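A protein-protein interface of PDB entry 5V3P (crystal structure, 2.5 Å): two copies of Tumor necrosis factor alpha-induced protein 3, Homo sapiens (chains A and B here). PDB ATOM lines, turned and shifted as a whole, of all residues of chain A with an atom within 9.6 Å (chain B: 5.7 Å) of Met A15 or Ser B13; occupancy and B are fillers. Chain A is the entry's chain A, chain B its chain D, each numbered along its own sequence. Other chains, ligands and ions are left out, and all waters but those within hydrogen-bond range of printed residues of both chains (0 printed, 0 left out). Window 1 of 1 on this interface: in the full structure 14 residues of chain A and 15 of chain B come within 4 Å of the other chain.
The backbone carbonyl oxygen (O) of Ser A13 lies within hydrogen-bond range of the backbone NH (N) of Met B15, 3.4 Å away.
The side-chain amide oxygen (OD1) of Asn B14 sits close to the side-chain amide oxygen (OD1) of Asn A14 (3.3 Å).
The backbone NH (N) of Met A15 is in hydrogen-bond range of the backbone carbonyl oxygen (O) of Ser B13, 3.3 Å away.
N of Arg A16 sits at hydrogen-bond distance from O of Ser B13 (3.0 Å).
NE of Arg A16 lies within salt-bridge range of OD1 of Asp B344 (3.9 Å).
The side-chain sulfur of Met B15 lies close to the backbone carbonyl oxygen of Leu A12 (3.4 Å).
SD of Met A15 lies close to O of Leu B12 (3.2 Å).
O of Leu A10 is in hydrogen-bond range of OG of Ser A13.
OD1 of Asn A14 lies within hydrogen-bond range of N of Lys A17 (3.1 Å).
The side-chain carboxylate of Asp A344 sits at hydrogen-bond distance from the side-chain amide nitrogen of Asn A14 (2.9 Å).
The backbone carbonyl oxygen (O) of Leu B10 is in hydrogen-bond range of the side-chain hydroxyl (OG) of Ser B13 (2.7 Å).
The side-chain carboxylate (OD2) of Asp B344 sits at hydrogen-bond distance from the side-chain amide nitrogen (ND2) of Asn B14, 2.9 Å away.
Pro B7 touches Met A15.
O of Met A15 touches CD2 of Leu B348, at 3.3 Å.
Leu B348 touches Arg A16 (CD2 to N, 3.6 Å).
Val A19 touches Leu B348.
Met B15 touches Leu A348 (O to CD2, 3.5 Å).
Of chain B, only Pro B7 (3.95 Å), Leu B12 (3.2 Å), Ser B13 (3.3 Å) and Leu B348 (3.3 Å) come within 4 Å of Met A15.
Of the printed residues of chain B, Arg A16 touches Ser B13 (3.0 Å), Asp B344 (3.2 Å) and Leu B348 (3.6 Å).
Of the printed residues of chain B, Val A19 touches Leu B348.
Glu A23 touches none of the printed residues of chain B.
Ala B9 touches none of the printed residues of chain A.
Printed residues of chain A within 4 Å of Leu B12: Met A15 (3.2 Å).
Printed residues of chain A within 4 Å of Ser B13: Met A15 and Arg A16.
Asn B14 touches just one residue of chain A: Asn A14.
Of the printed residues of chain A, Met B15 touches Leu A12 (3.4 Å), Ser A13 (3.4 Å) and Leu A348 (3.5 Å).
Of the printed residues of chain A, Asp B344 touches Arg A16 (3.2 Å).
The nearest printed residue of chain B that does not touch Met A15 is Asn B14 (4.6 Å).
The nearest printed residue of chain A that does not touch Ser B13 is Asn A14 (4.01 Å).
The nearest printed residue of chain A that does not touch Pro B7 is Leu A12 (6.8 Å).
Hydrophobic or aromatic side chains of chain A that line the printed part of chain B: Met A15, Val A19 and Leu A348.
Of the 13 printed residues of chain B, 7 touch a printed residue of chain A.
Hydrophobic or aromatic side chains of chain B within 4 Å of the printed part of chain A: Pro B7, Met B15 and Leu B348.
Along chain B the printed residues that touch a printed residue of chain A span positions 7 to 348.
Leu A12 touches Met B15, and with the chains exchanged Met A15 touches Leu B12.
Asn B14 touches its own counterpart, Asn A14.
Met A15 touches Pro B7, but with the chains exchanged Pro A7 does not touch Met B15 (4.1 Å).
Met A15 touches Leu B348, and with the chains exchanged Leu A348 touches Met B15.
Positions printed for both chains: 7, 9, 10, 11, 12, 13, 14, 15, 341, 344, 345 and 348.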
ATOM      1  N   PRO A   7       8.816  -7.296 -18.525  1.00  0.00           N
ATOM      2  CA  PRO A   7       7.377  -7.221 -18.858  1.00  0.00           C
ATOM      3  C   PRO A   7       6.851  -5.810 -19.108  1.00  0.00           C
ATOM      4  O   PRO A   7       7.472  -4.829 -18.701  1.00  0.00           O
ATOM      5  CB  PRO A   7       6.701  -7.871 -17.652  1.00  0.00           C
ATOM      6  CG  PRO A   7       7.689  -7.756 -16.529  1.00  0.00           C
ATOM      7  CD  PRO A   7       9.056  -7.553 -17.094  1.00  0.00           C
ATOM      8  N   ALA A   9       4.101  -4.170 -18.116  1.00  0.00           N
ATOM      9  CA  ALA A   9       3.324  -3.519 -17.071  1.00  0.00           C
ATOM     10  C   ALA A   9       3.961  -3.795 -15.713  1.00  0.00           C
ATOM     11  O   ALA A   9       4.575  -4.847 -15.510  1.00  0.00           O
ATOM     12  CB  ALA A   9       1.881  -4.003 -17.101  1.00  0.00           C
ATOM     13  N   LEU A  10       3.815  -2.860 -14.779  1.00  0.00           N
ATOM     14  CA  LEU A  10       4.327  -3.062 -13.422  1.00  0.00           C
ATOM     15  C   LEU A  10       3.739  -4.313 -12.770  1.00  0.00           C
ATOM     16  O   LEU A  10       4.459  -5.050 -12.103  1.00  0.00           O
ATOM     17  CB  LEU A  10       4.021  -1.848 -12.538  1.00  0.00           C
ATOM     18  CG  LEU A  10       4.872  -0.596 -12.811  1.00  0.00           C
ATOM     19  CD1 LEU A  10       4.480   0.498 -11.826  1.00  0.00           C
ATOM     20  CD2 LEU A  10       6.394  -0.853 -12.748  1.00  0.00           C
ATOM     21  N   TYR A  11       2.436  -4.563 -12.980  1.00  0.00           N
ATOM     22  CA  TYR A  11       1.755  -5.636 -12.276  1.00  0.00           C
ATOM     23  C   TYR A  11       2.188  -7.050 -12.670  1.00  0.00           C
ATOM     24  O   TYR A  11       2.070  -7.976 -11.885  1.00  0.00           O
ATOM     25  CB  TYR A  11       0.245  -5.474 -12.417  1.00  0.00           C
ATOM     26  CG  TYR A  11      -0.366  -6.141 -13.634  1.00  0.00           C
ATOM     27  CD1 TYR A  11      -0.488  -5.457 -14.843  1.00  0.00           C
ATOM     28  CD2 TYR A  11      -0.850  -7.451 -13.565  1.00  0.00           C
ATOM     29  CE1 TYR A  11      -1.052  -6.068 -15.959  1.00  0.00           C
ATOM     30  CE2 TYR A  11      -1.453  -8.060 -14.642  1.00  0.00           C
ATOM     31  CZ  TYR A  11      -1.555  -7.380 -15.841  1.00  0.00           C
ATOM     32  OH  TYR A  11      -2.131  -8.035 -16.915  1.00  0.00           O
ATOM     33  N   LEU A  12       2.671  -7.214 -13.901  1.00  0.00           N
ATOM     34  CA  LEU A  12       3.113  -8.514 -14.375  1.00  0.00           C
ATOM     35  C   LEU A  12       4.354  -9.026 -13.656  1.00  0.00           C
ATOM     36  O   LEU A  12       4.677 -10.196 -13.784  1.00  0.00           O
ATOM     37  CB  LEU A  12       3.340  -8.471 -15.893  1.00  0.00           C
ATOM     38  CG  LEU A  12       2.063  -8.580 -16.750  1.00  0.00           C
ATOM     39  CD1 LEU A  12       2.466  -8.509 -18.230  1.00  0.00           C
ATOM     40  CD2 LEU A  12       1.297  -9.882 -16.551  1.00  0.00           C
ATOM     41  N   SER A  13       5.058  -8.150 -12.931  1.00  0.00           N
ATOM     42  CA  SER A  13       6.217  -8.542 -12.111  1.00  0.00           C
ATOM     43  C   SER A  13       5.857  -9.379 -10.888  1.00  0.00           C
ATOM     44  O   SER A  13       6.744 -10.002 -10.296  1.00  0.00           O
ATOM     45  CB  SER A  13       6.969  -7.308 -11.646  1.00  0.00           C
ATOM     46  OG  SER A  13       6.194  -6.570 -10.707  1.00  0.00           O
ATOM     47  N   ASN A  14       4.594  -9.361 -10.481  1.00  0.00           N
ATOM     48  CA  ASN A  14       4.129 -10.168  -9.357  1.00  0.00           C
ATOM     49  C   ASN A  14       2.600 -10.196  -9.385  1.00  0.00           C
ATOM     50  O   ASN A  14       1.919  -9.470  -8.662  1.00  0.00           O
ATOM     51  CB  ASN A  14       4.662  -9.629  -8.039  1.00  0.00           C
ATOM     52  CG  ASN A  14       4.325 -10.486  -6.864  1.00  0.00           C
ATOM     53  OD1 ASN A  14       3.557 -11.432  -6.970  1.00  0.00           O
ATOM     54  ND2 ASN A  14       4.890 -10.133  -5.707  1.00  0.00           N
ATOM     55  N   MET A  15       2.090 -11.052 -10.266  1.00  0.00           N
ATOM     56  CA  MET A  15       0.661 -11.178 -10.518  1.00  0.00           C
ATOM     57  C   MET A  15      -0.126 -11.578  -9.292  1.00  0.00           C
ATOM     58  O   MET A  15      -1.280 -11.185  -9.149  1.00  0.00           O
ATOM     59  CB  MET A  15       0.416 -12.183 -11.654  1.00  0.00           C
ATOM     60  CG  MET A  15       0.859 -11.682 -13.016  1.00  0.00           C
ATOM     61  SD  MET A  15       0.666 -13.001 -14.221  1.00  0.00           S
ATOM     62  CE  MET A  15      -1.042 -12.644 -14.679  1.00  0.00           C
ATOM     63  N   ARG A  16       0.498 -12.353  -8.417  1.00  0.00           N
ATOM     64  CA  ARG A  16      -0.074 -12.732  -7.130  1.00  0.00           C
ATOM     65  C   ARG A  16      -0.315 -11.518  -6.248  1.00  0.00           C
ATOM     66  O   ARG A  16      -1.308 -11.449  -5.541  1.00  0.00           O
ATOM     67  CB  ARG A  16       0.845 -13.701  -6.399  1.00  0.00           C
ATOM     68  CG  ARG A  16       0.591 -13.841  -4.908  1.00  0.00           C
ATOM     69  CD  ARG A  16      -0.667 -14.633  -4.643  1.00  0.00           C
ATOM     70  NE  ARG A  16      -1.010 -14.646  -3.212  1.00  0.00           N
ATOM     71  CZ  ARG A  16      -2.013 -13.956  -2.645  1.00  0.00           C
ATOM     72  NH1 ARG A  16      -2.811 -13.167  -3.369  1.00  0.00           N
ATOM     73  NH2 ARG A  16      -2.202 -14.045  -1.331  1.00  0.00           N
ATOM     74  N   LYS A  17       0.628 -10.592  -6.240  1.00  0.00           N
ATOM     75  CA  LYS A  17       0.497  -9.379  -5.440  1.00  0.00           C
ATOM     76  C   LYS A  17      -0.561  -8.436  -6.028  1.00  0.00           C
ATOM     77  O   LYS A  17      -1.382  -7.870  -5.286  1.00  0.00           O
ATOM     78  CB  LYS A  17       1.862  -8.697  -5.333  1.00  0.00           C
ATOM     79  CG  LYS A  17       1.900  -7.487  -4.430  1.00  0.00           C
ATOM     80  CD  LYS A  17       3.294  -6.921  -4.357  1.00  0.00           C
ATOM     81  CE  LYS A  17       4.129  -7.513  -3.225  1.00  0.00           C
ATOM     82  NZ  LYS A  17       5.423  -6.758  -3.109  1.00  0.00           N
ATOM     83  N   ALA A  18      -0.555  -8.294  -7.349  1.00  0.00           N
ATOM     84  CA  ALA A  18      -1.590  -7.527  -8.032  1.00  0.00           C
ATOM     85  C   ALA A  18      -2.980  -8.085  -7.739  1.00  0.00           C
ATOM     86  O   ALA A  18      -3.916  -7.304  -7.522  1.00  0.00           O
ATOM     87  CB  ALA A  18      -1.352  -7.487  -9.522  1.00  0.00           C
ATOM     88  N   VAL A  19      -3.136  -9.408  -7.703  1.00  0.00           N
ATOM     89  CA  VAL A  19      -4.434  -9.999  -7.331  1.00  0.00           C
ATOM     90  C   VAL A  19      -4.814  -9.594  -5.902  1.00  0.00           C
ATOM     91  O   VAL A  19      -5.949  -9.199  -5.674  1.00  0.00           O
ATOM     92  CB  VAL A  19      -4.461 -11.554  -7.522  1.00  0.00           C
ATOM     93  CG1 VAL A  19      -5.426 -12.287  -6.582  1.00  0.00           C
ATOM     94  CG2 VAL A  19      -4.669 -11.896  -8.994  1.00  0.00           C
ATOM     95  N   LYS A  20      -3.871  -9.648  -4.957  1.00  0.00           N
ATOM     96  CA  LYS A  20      -4.114  -9.196  -3.580  1.00  0.00           C
ATOM     97  C   LYS A  20      -4.646  -7.780  -3.506  1.00  0.00           C
ATOM     98  O   LYS A  20      -5.618  -7.523  -2.804  1.00  0.00           O
ATOM     99  CB  LYS A  20      -2.827  -9.303  -2.781  1.00  0.00           C
ATOM    100  CG  LYS A  20      -2.858  -8.781  -1.353  1.00  0.00           C
ATOM    101  CD  LYS A  20      -1.625  -9.316  -0.587  1.00  0.00           C
ATOM    102  CE  LYS A  20      -0.751  -8.270   0.148  1.00  0.00           C
ATOM    103  NZ  LYS A  20       0.692  -8.668  -0.068  1.00  0.00           N
ATOM    104  N   ILE A  21      -4.020  -6.876  -4.257  1.00  0.00           N
ATOM    105  CA  ILE A  21      -4.437  -5.477  -4.368  1.00  0.00           C
ATOM    106  C   ILE A  21      -5.853  -5.386  -4.921  1.00  0.00           C
ATOM    107  O   ILE A  21      -6.699  -4.717  -4.359  1.00  0.00           O
ATOM    108  CB  ILE A  21      -3.472  -4.673  -5.274  1.00  0.00           C
ATOM    109  CG1 ILE A  21      -2.108  -4.505  -4.599  1.00  0.00           C
ATOM    110  CG2 ILE A  21      -4.048  -3.290  -5.580  1.00  0.00           C
ATOM    111  CD1 ILE A  21      -0.988  -4.064  -5.513  1.00  0.00           C
ATOM    112  N   ARG A  22      -6.106  -6.069  -6.031  1.00  0.00           N
ATOM    113  CA  ARG A  22      -7.425  -6.024  -6.662  1.00  0.00           C
ATOM    114  C   ARG A  22      -8.534  -6.711  -5.858  1.00  0.00           C
ATOM    115  O   ARG A  22      -9.722  -6.460  -6.113  1.00  0.00           O
ATOM    116  CB  ARG A  22      -7.366  -6.609  -8.052  1.00  0.00           C
ATOM    117  CG  ARG A  22      -6.557  -5.739  -9.025  1.00  0.00           C
ATOM    118  CD  ARG A  22      -6.898  -6.064 -10.481  1.00  0.00           C
ATOM    119  NE  ARG A  22      -6.935  -7.523 -10.672  1.00  0.00           N
ATOM    120  CZ  ARG A  22      -5.895  -8.272 -11.069  1.00  0.00           C
ATOM    121  NH1 ARG A  22      -4.697  -7.731 -11.396  1.00  0.00           N
ATOM    122  NH2 ARG A  22      -6.083  -9.597 -11.132  1.00  0.00           N
ATOM    123  N   GLU A  23      -8.163  -7.584  -4.912  1.00  0.00           N
ATOM    124  CA  GLU A  23      -9.146  -8.151  -3.998  1.00  0.00           C
ATOM    125  C   GLU A  23      -9.446  -7.230  -2.850  1.00  0.00           C
ATOM    126  O   GLU A  23     -10.567  -7.204  -2.366  1.00  0.00           O
ATOM    127  CB  GLU A  23      -8.713  -9.531  -3.464  1.00  0.00           C
ATOM    128  CG  GLU A  23      -8.980 -10.664  -4.454  1.00  0.00           C
ATOM    129  CD  GLU A  23      -9.296 -12.027  -3.835  1.00  0.00           C
ATOM    130  OE1 GLU A  23      -9.208 -12.188  -2.594  1.00  0.00           O
ATOM    131  OE2 GLU A  23      -9.670 -12.888  -4.632  1.00  0.00           O
ATOM    132  N   GLY A 114      -0.864   0.844  -8.872  1.00  0.00           N
ATOM    133  CA  GLY A 114       0.014   0.137  -9.820  1.00  0.00           C
ATOM    134  C   GLY A 114      -0.640  -1.004 -10.585  1.00  0.00           C
ATOM    135  O   GLY A 114       0.056  -1.801 -11.277  1.00  0.00           O
ATOM    136  N   VAL A 115      -1.968  -1.103 -10.475  1.00  0.00           N
ATOM    137  CA  VAL A 115      -2.744  -2.092 -11.201  1.00  0.00           C
ATOM    138  C   VAL A 115      -3.804  -1.352 -11.979  1.00  0.00           C
ATOM    139  O   VAL A 115      -4.230  -0.234 -11.589  1.00  0.00           O
ATOM    140  CB  VAL A 115      -3.434  -3.108 -10.256  1.00  0.00           C
ATOM    141  CG1 VAL A 115      -2.365  -3.902  -9.453  1.00  0.00           C
ATOM    142  CG2 VAL A 115      -4.420  -2.414  -9.293  1.00  0.00           C
ATOM    143  N   THR A 118      -8.969  -3.975 -13.998  1.00  0.00           N
ATOM    144  CA  THR A 118      -9.287  -5.183 -14.780  1.00  0.00           C
ATOM    145  C   THR A 118     -10.579  -5.854 -14.308  1.00  0.00           C
ATOM    146  O   THR A 118     -11.283  -6.473 -15.110  1.00  0.00           O
ATOM    147  CB  THR A 118      -8.123  -6.192 -14.724  1.00  0.00           C
ATOM    148  OG1 THR A 118      -6.898  -5.545 -15.042  1.00  0.00           O
ATOM    149  CG2 THR A 118      -8.357  -7.349 -15.686  1.00  0.00           C
ATOM    150  N   ASP A 119     -10.876  -5.729 -13.015  1.00  0.00           N
ATOM    151  CA  ASP A 119     -12.099  -6.270 -12.393  1.00  0.00           C
ATOM    152  C   ASP A 119     -13.258  -5.259 -12.348  1.00  0.00           C
ATOM    153  O   ASP A 119     -14.282  -5.513 -11.706  1.00  0.00           O
ATOM    154  CB  ASP A 119     -11.795  -6.770 -10.975  1.00  0.00           C
ATOM    155  CG  ASP A 119     -10.689  -7.857 -10.954  1.00  0.00           C
ATOM    156  OD1 ASP A 119     -10.553  -8.590 -11.956  1.00  0.00           O
ATOM    157  OD2 ASP A 119      -9.980  -8.014  -9.946  1.00  0.00           O
ATOM    158  N   LEU A 341       4.102  -3.008  -5.995  1.00  0.00           N
ATOM    159  CA  LEU A 341       4.571  -3.622  -7.231  1.00  0.00           C
ATOM    160  C   LEU A 341       5.864  -3.050  -7.805  1.00  0.00           C
ATOM    161  O   LEU A 341       6.583  -3.754  -8.520  1.00  0.00           O
ATOM    162  CB  LEU A 341       3.484  -3.524  -8.297  1.00  0.00           C
ATOM    163  CG  LEU A 341       2.310  -4.434  -8.008  1.00  0.00           C
ATOM    164  CD1 LEU A 341       1.034  -3.928  -8.695  1.00  0.00           C
ATOM    165  CD2 LEU A 341       2.640  -5.899  -8.362  1.00  0.00           C
ATOM    166  N   ASP A 344       9.074  -4.778  -6.608  1.00  0.00           N
ATOM    167  CA  ASP A 344       9.177  -6.049  -7.330  1.00  0.00           C
ATOM    168  C   ASP A 344       9.673  -5.904  -8.757  1.00  0.00           C
ATOM    169  O   ASP A 344      10.463  -6.728  -9.208  1.00  0.00           O
ATOM    170  CB  ASP A 344       7.845  -6.786  -7.352  1.00  0.00           C
ATOM    171  CG  ASP A 344       7.487  -7.386  -6.012  1.00  0.00           C
ATOM    172  OD1 ASP A 344       8.411  -7.645  -5.189  1.00  0.00           O
ATOM    173  OD2 ASP A 344       6.278  -7.606  -5.778  1.00  0.00           O
ATOM    174  N   TYR A 345       9.206  -4.883  -9.473  1.00  0.00           N
ATOM    175  CA  TYR A 345       9.628  -4.684 -10.861  1.00  0.00           C
ATOM    176  C   TYR A 345      11.097  -4.254 -10.892  1.00  0.00           C
ATOM    177  O   TYR A 345      11.853  -4.674 -11.774  1.00  0.00           O
ATOM    178  CB  TYR A 345       8.737  -3.661 -11.582  1.00  0.00           C
ATOM    179  CG  TYR A 345       8.833  -3.711 -13.098  1.00  0.00           C
ATOM    180  CD1 TYR A 345       9.920  -3.143 -13.769  1.00  0.00           C
ATOM    181  CD2 TYR A 345       7.833  -4.305 -13.865  1.00  0.00           C
ATOM    182  CE1 TYR A 345      10.002  -3.175 -15.158  1.00  0.00           C
ATOM    183  CE2 TYR A 345       7.916  -4.346 -15.251  1.00  0.00           C
ATOM    184  CZ  TYR A 345       9.011  -3.778 -15.895  1.00  0.00           C
ATOM    185  OH  TYR A 345       9.102  -3.807 -17.281  1.00  0.00           O
ATOM    186  N   LEU A 348      13.427  -7.292 -10.753  1.00  0.00           N
ATOM    187  CA  LEU A 348      13.608  -7.891 -12.092  1.00  0.00           C
ATOM    188  C   LEU A 348      14.611  -7.097 -12.920  1.00  0.00           C
ATOM    189  O   LEU A 348      15.416  -7.679 -13.630  1.00  0.00           O
ATOM    190  CB  LEU A 348      12.309  -7.946 -12.894  1.00  0.00           C
ATOM    191  CG  LEU A 348      11.070  -8.635 -12.367  1.00  0.00           C
ATOM    192  CD1 LEU A 348      10.049  -8.752 -13.495  1.00  0.00           C
ATOM    193  CD2 LEU A 348      11.337  -9.981 -11.737  1.00  0.00           C
ATOM    194  N   VAL B   5      -6.037 -15.402 -20.165  1.00  0.00           N
ATOM    195  CA  VAL B   5      -6.091 -14.619 -18.887  1.00  0.00           C
ATOM    196  C   VAL B   5      -5.199 -15.214 -17.790  1.00  0.00           C
ATOM    197  O   VAL B   5      -4.392 -14.483 -17.196  1.00  0.00           O
ATOM    198  CB  VAL B   5      -7.558 -14.402 -18.430  1.00  0.00           C
ATOM    199  CG1 VAL B   5      -8.174 -15.621 -17.734  1.00  0.00           C
ATOM    200  CG2 VAL B   5      -7.719 -13.119 -17.591  1.00  0.00           C
ATOM    201  N   PRO B   7      -1.754 -17.232 -16.899  1.00  0.00           N
ATOM    202  CA  PRO B   7      -0.470 -17.324 -17.596  1.00  0.00           C
ATOM    203  C   PRO B   7      -0.027 -18.757 -17.941  1.00  0.00           C
ATOM    204  O   PRO B   7      -0.514 -19.727 -17.340  1.00  0.00           O
ATOM    205  CB  PRO B   7       0.519 -16.663 -16.628  1.00  0.00           C
ATOM    206  CG  PRO B   7      -0.118 -16.725 -15.290  1.00  0.00           C
ATOM    207  CD  PRO B   7      -1.594 -16.913 -15.463  1.00  0.00           C
ATOM    208  N   ALA B   9       2.887 -20.403 -17.700  1.00  0.00           N
ATOM    209  CA  ALA B   9       3.872 -21.098 -16.869  1.00  0.00           C
ATOM    210  C   ALA B   9       3.636 -20.747 -15.394  1.00  0.00           C
ATOM    211  O   ALA B   9       3.111 -19.671 -15.075  1.00  0.00           O
ATOM    212  CB  ALA B   9       5.272 -20.695 -17.282  1.00  0.00           C
ATOM    213  N   LEU B  10       4.010 -21.652 -14.492  1.00  0.00           N
ATOM    214  CA  LEU B  10       3.892 -21.392 -13.066  1.00  0.00           C
ATOM    215  C   LEU B  10       4.639 -20.130 -12.627  1.00  0.00           C
ATOM    216  O   LEU B  10       4.136 -19.357 -11.822  1.00  0.00           O
ATOM    217  CB  LEU B  10       4.388 -22.586 -12.239  1.00  0.00           C
ATOM    218  CG  LEU B  10       3.505 -23.820 -12.215  1.00  0.00           C
ATOM    219  CD1 LEU B  10       4.162 -24.878 -11.340  1.00  0.00           C
ATOM    220  CD2 LEU B  10       2.083 -23.525 -11.733  1.00  0.00           C
ATOM    221  N   TYR B  11       5.826 -19.920 -13.173  1.00  0.00           N
ATOM    222  CA  TYR B  11       6.711 -18.846 -12.704  1.00  0.00           C
ATOM    223  C   TYR B  11       6.212 -17.435 -13.035  1.00  0.00           C
ATOM    224  O   TYR B  11       6.550 -16.488 -12.343  1.00  0.00           O
ATOM    225  CB  TYR B  11       8.128 -19.029 -13.233  1.00  0.00           C
ATOM    226  CG  TYR B  11       8.389 -18.458 -14.604  1.00  0.00           C
ATOM    227  CD1 TYR B  11       8.167 -19.216 -15.767  1.00  0.00           C
ATOM    228  CD2 TYR B  11       8.898 -17.165 -14.740  1.00  0.00           C
ATOM    229  CE1 TYR B  11       8.435 -18.689 -17.021  1.00  0.00           C
ATOM    230  CE2 TYR B  11       9.216 -16.645 -15.985  1.00  0.00           C
ATOM    231  CZ  TYR B  11       8.968 -17.395 -17.123  1.00  0.00           C
ATOM    232  OH  TYR B  11       9.243 -16.822 -18.350  1.00  0.00           O
ATOM    233  N   LEU B  12       5.415 -17.303 -14.100  1.00  0.00           N
ATOM    234  CA  LEU B  12       4.885 -16.014 -14.489  1.00  0.00           C
ATOM    235  C   LEU B  12       3.896 -15.431 -13.480  1.00  0.00           C
ATOM    236  O   LEU B  12       3.576 -14.264 -13.556  1.00  0.00           O
ATOM    237  CB  LEU B  12       4.246 -16.102 -15.886  1.00  0.00           C
ATOM    238  CG  LEU B  12       5.260 -16.125 -17.062  1.00  0.00           C
ATOM    239  CD1 LEU B  12       4.490 -16.279 -18.369  1.00  0.00           C
ATOM    240  CD2 LEU B  12       6.081 -14.839 -17.172  1.00  0.00           C
ATOM    241  N   SER B  13       3.393 -16.261 -12.557  1.00  0.00           N
ATOM    242  CA  SER B  13       2.513 -15.813 -11.468  1.00  0.00           C
ATOM    243  C   SER B  13       3.203 -14.944 -10.415  1.00  0.00           C
ATOM    244  O   SER B  13       2.538 -14.263  -9.623  1.00  0.00           O
ATOM    245  CB  SER B  13       1.909 -17.011 -10.753  1.00  0.00           C
ATOM    246  OG  SER B  13       2.915 -17.736 -10.034  1.00  0.00           O
ATOM    247  N   ASN B  14       4.531 -14.984 -10.369  1.00  0.00           N
ATOM    248  CA  ASN B  14       5.304 -14.167  -9.437  1.00  0.00           C
ATOM    249  C   ASN B  14       6.749 -14.160  -9.889  1.00  0.00           C
ATOM    250  O   ASN B  14       7.600 -14.869  -9.348  1.00  0.00           O
ATOM    251  CB  ASN B  14       5.147 -14.672  -8.009  1.00  0.00           C
ATOM    252  CG  ASN B  14       5.784 -13.765  -7.001  1.00  0.00           C
ATOM    253  OD1 ASN B  14       6.497 -12.822  -7.351  1.00  0.00           O
ATOM    254  ND2 ASN B  14       5.570 -14.075  -5.719  1.00  0.00           N
ATOM    255  N   MET B  15       7.002 -13.340 -10.914  1.00  0.00           N
ATOM    256  CA  MET B  15       8.304 -13.250 -11.556  1.00  0.00           C
ATOM    257  C   MET B  15       9.400 -12.819 -10.595  1.00  0.00           C
ATOM    258  O   MET B  15      10.554 -13.217 -10.759  1.00  0.00           O
ATOM    259  CB  MET B  15       8.231 -12.297 -12.746  1.00  0.00           C
ATOM    260  CG  MET B  15       7.487 -12.880 -13.943  1.00  0.00           C
ATOM    261  SD  MET B  15       7.369 -11.641 -15.268  1.00  0.00           S
ATOM    262  CE  MET B  15       8.987 -11.965 -16.026  1.00  0.00           C
ATOM    263  N   LEU B 341       6.197 -21.235  -5.977  1.00  0.00           N
ATOM    264  CA  LEU B 341       5.404 -20.626  -7.051  1.00  0.00           C
ATOM    265  C   LEU B 341       3.998 -21.189  -7.234  1.00  0.00           C
ATOM    266  O   LEU B 341       3.115 -20.484  -7.737  1.00  0.00           O
ATOM    267  CB  LEU B 341       6.155 -20.742  -8.372  1.00  0.00           C
ATOM    268  CG  LEU B 341       7.382 -19.816  -8.387  1.00  0.00           C
ATOM    269  CD1 LEU B 341       8.443 -20.309  -9.358  1.00  0.00           C
ATOM    270  CD2 LEU B 341       6.969 -18.404  -8.719  1.00  0.00           C
ATOM    271  N   ASP B 344       1.249 -19.369  -5.240  1.00  0.00           N
ATOM    272  CA  ASP B 344       0.960 -18.121  -5.948  1.00  0.00           C
ATOM    273  C   ASP B 344       0.094 -18.295  -7.185  1.00  0.00           C
ATOM    274  O   ASP B 344      -0.785 -17.473  -7.435  1.00  0.00           O
ATOM    275  CB  ASP B 344       2.240 -17.402  -6.361  1.00  0.00           C
ATOM    276  CG  ASP B 344       2.967 -16.781  -5.190  1.00  0.00           C
ATOM    277  OD1 ASP B 344       2.318 -16.473  -4.174  1.00  0.00           O
ATOM    278  OD2 ASP B 344       4.186 -16.568  -5.293  1.00  0.00           O
ATOM    279  N   TYR B 345       0.342 -19.337  -7.970  1.00  0.00           N
ATOM    280  CA  TYR B 345      -0.449 -19.570  -9.187  1.00  0.00           C
ATOM    281  C   TYR B 345      -1.876 -19.981  -8.798  1.00  0.00           C
ATOM    282  O   TYR B 345      -2.843 -19.576  -9.450  1.00  0.00           O
ATOM    283  CB  TYR B 345       0.198 -20.624 -10.092  1.00  0.00           C
ATOM    284  CG  TYR B 345      -0.317 -20.625 -11.525  1.00  0.00           C
ATOM    285  CD1 TYR B 345      -1.553 -21.190 -11.852  1.00  0.00           C
ATOM    286  CD2 TYR B 345       0.425 -20.074 -12.556  1.00  0.00           C
ATOM    287  CE1 TYR B 345      -2.024 -21.193 -13.162  1.00  0.00           C
ATOM    288  CE2 TYR B 345      -0.029 -20.080 -13.874  1.00  0.00           C
ATOM    289  CZ  TYR B 345      -1.249 -20.633 -14.172  1.00  0.00           C
ATOM    290  OH  TYR B 345      -1.708 -20.655 -15.480  1.00  0.00           O
ATOM    291  N   LEU B 348      -4.073 -16.913  -8.134  1.00  0.00           N
ATOM    292  CA  LEU B 348      -4.606 -16.348  -9.392  1.00  0.00           C
ATOM    293  C   LEU B 348      -5.812 -17.159  -9.879  1.00  0.00           C
ATOM    294  O   LEU B 348      -6.793 -16.585 -10.353  1.00  0.00           O
ATOM    295  CB  LEU B 348      -3.596 -16.336 -10.530  1.00  0.00           C
ATOM    296  CG  LEU B 348      -2.243 -15.653 -10.375  1.00  0.00           C
ATOM    297  CD1 LEU B 348      -1.559 -15.590 -11.761  1.00  0.00           C
ATOM    298  CD2 LEU B 348      -2.289 -14.294  -9.699  1.00  0.00           C
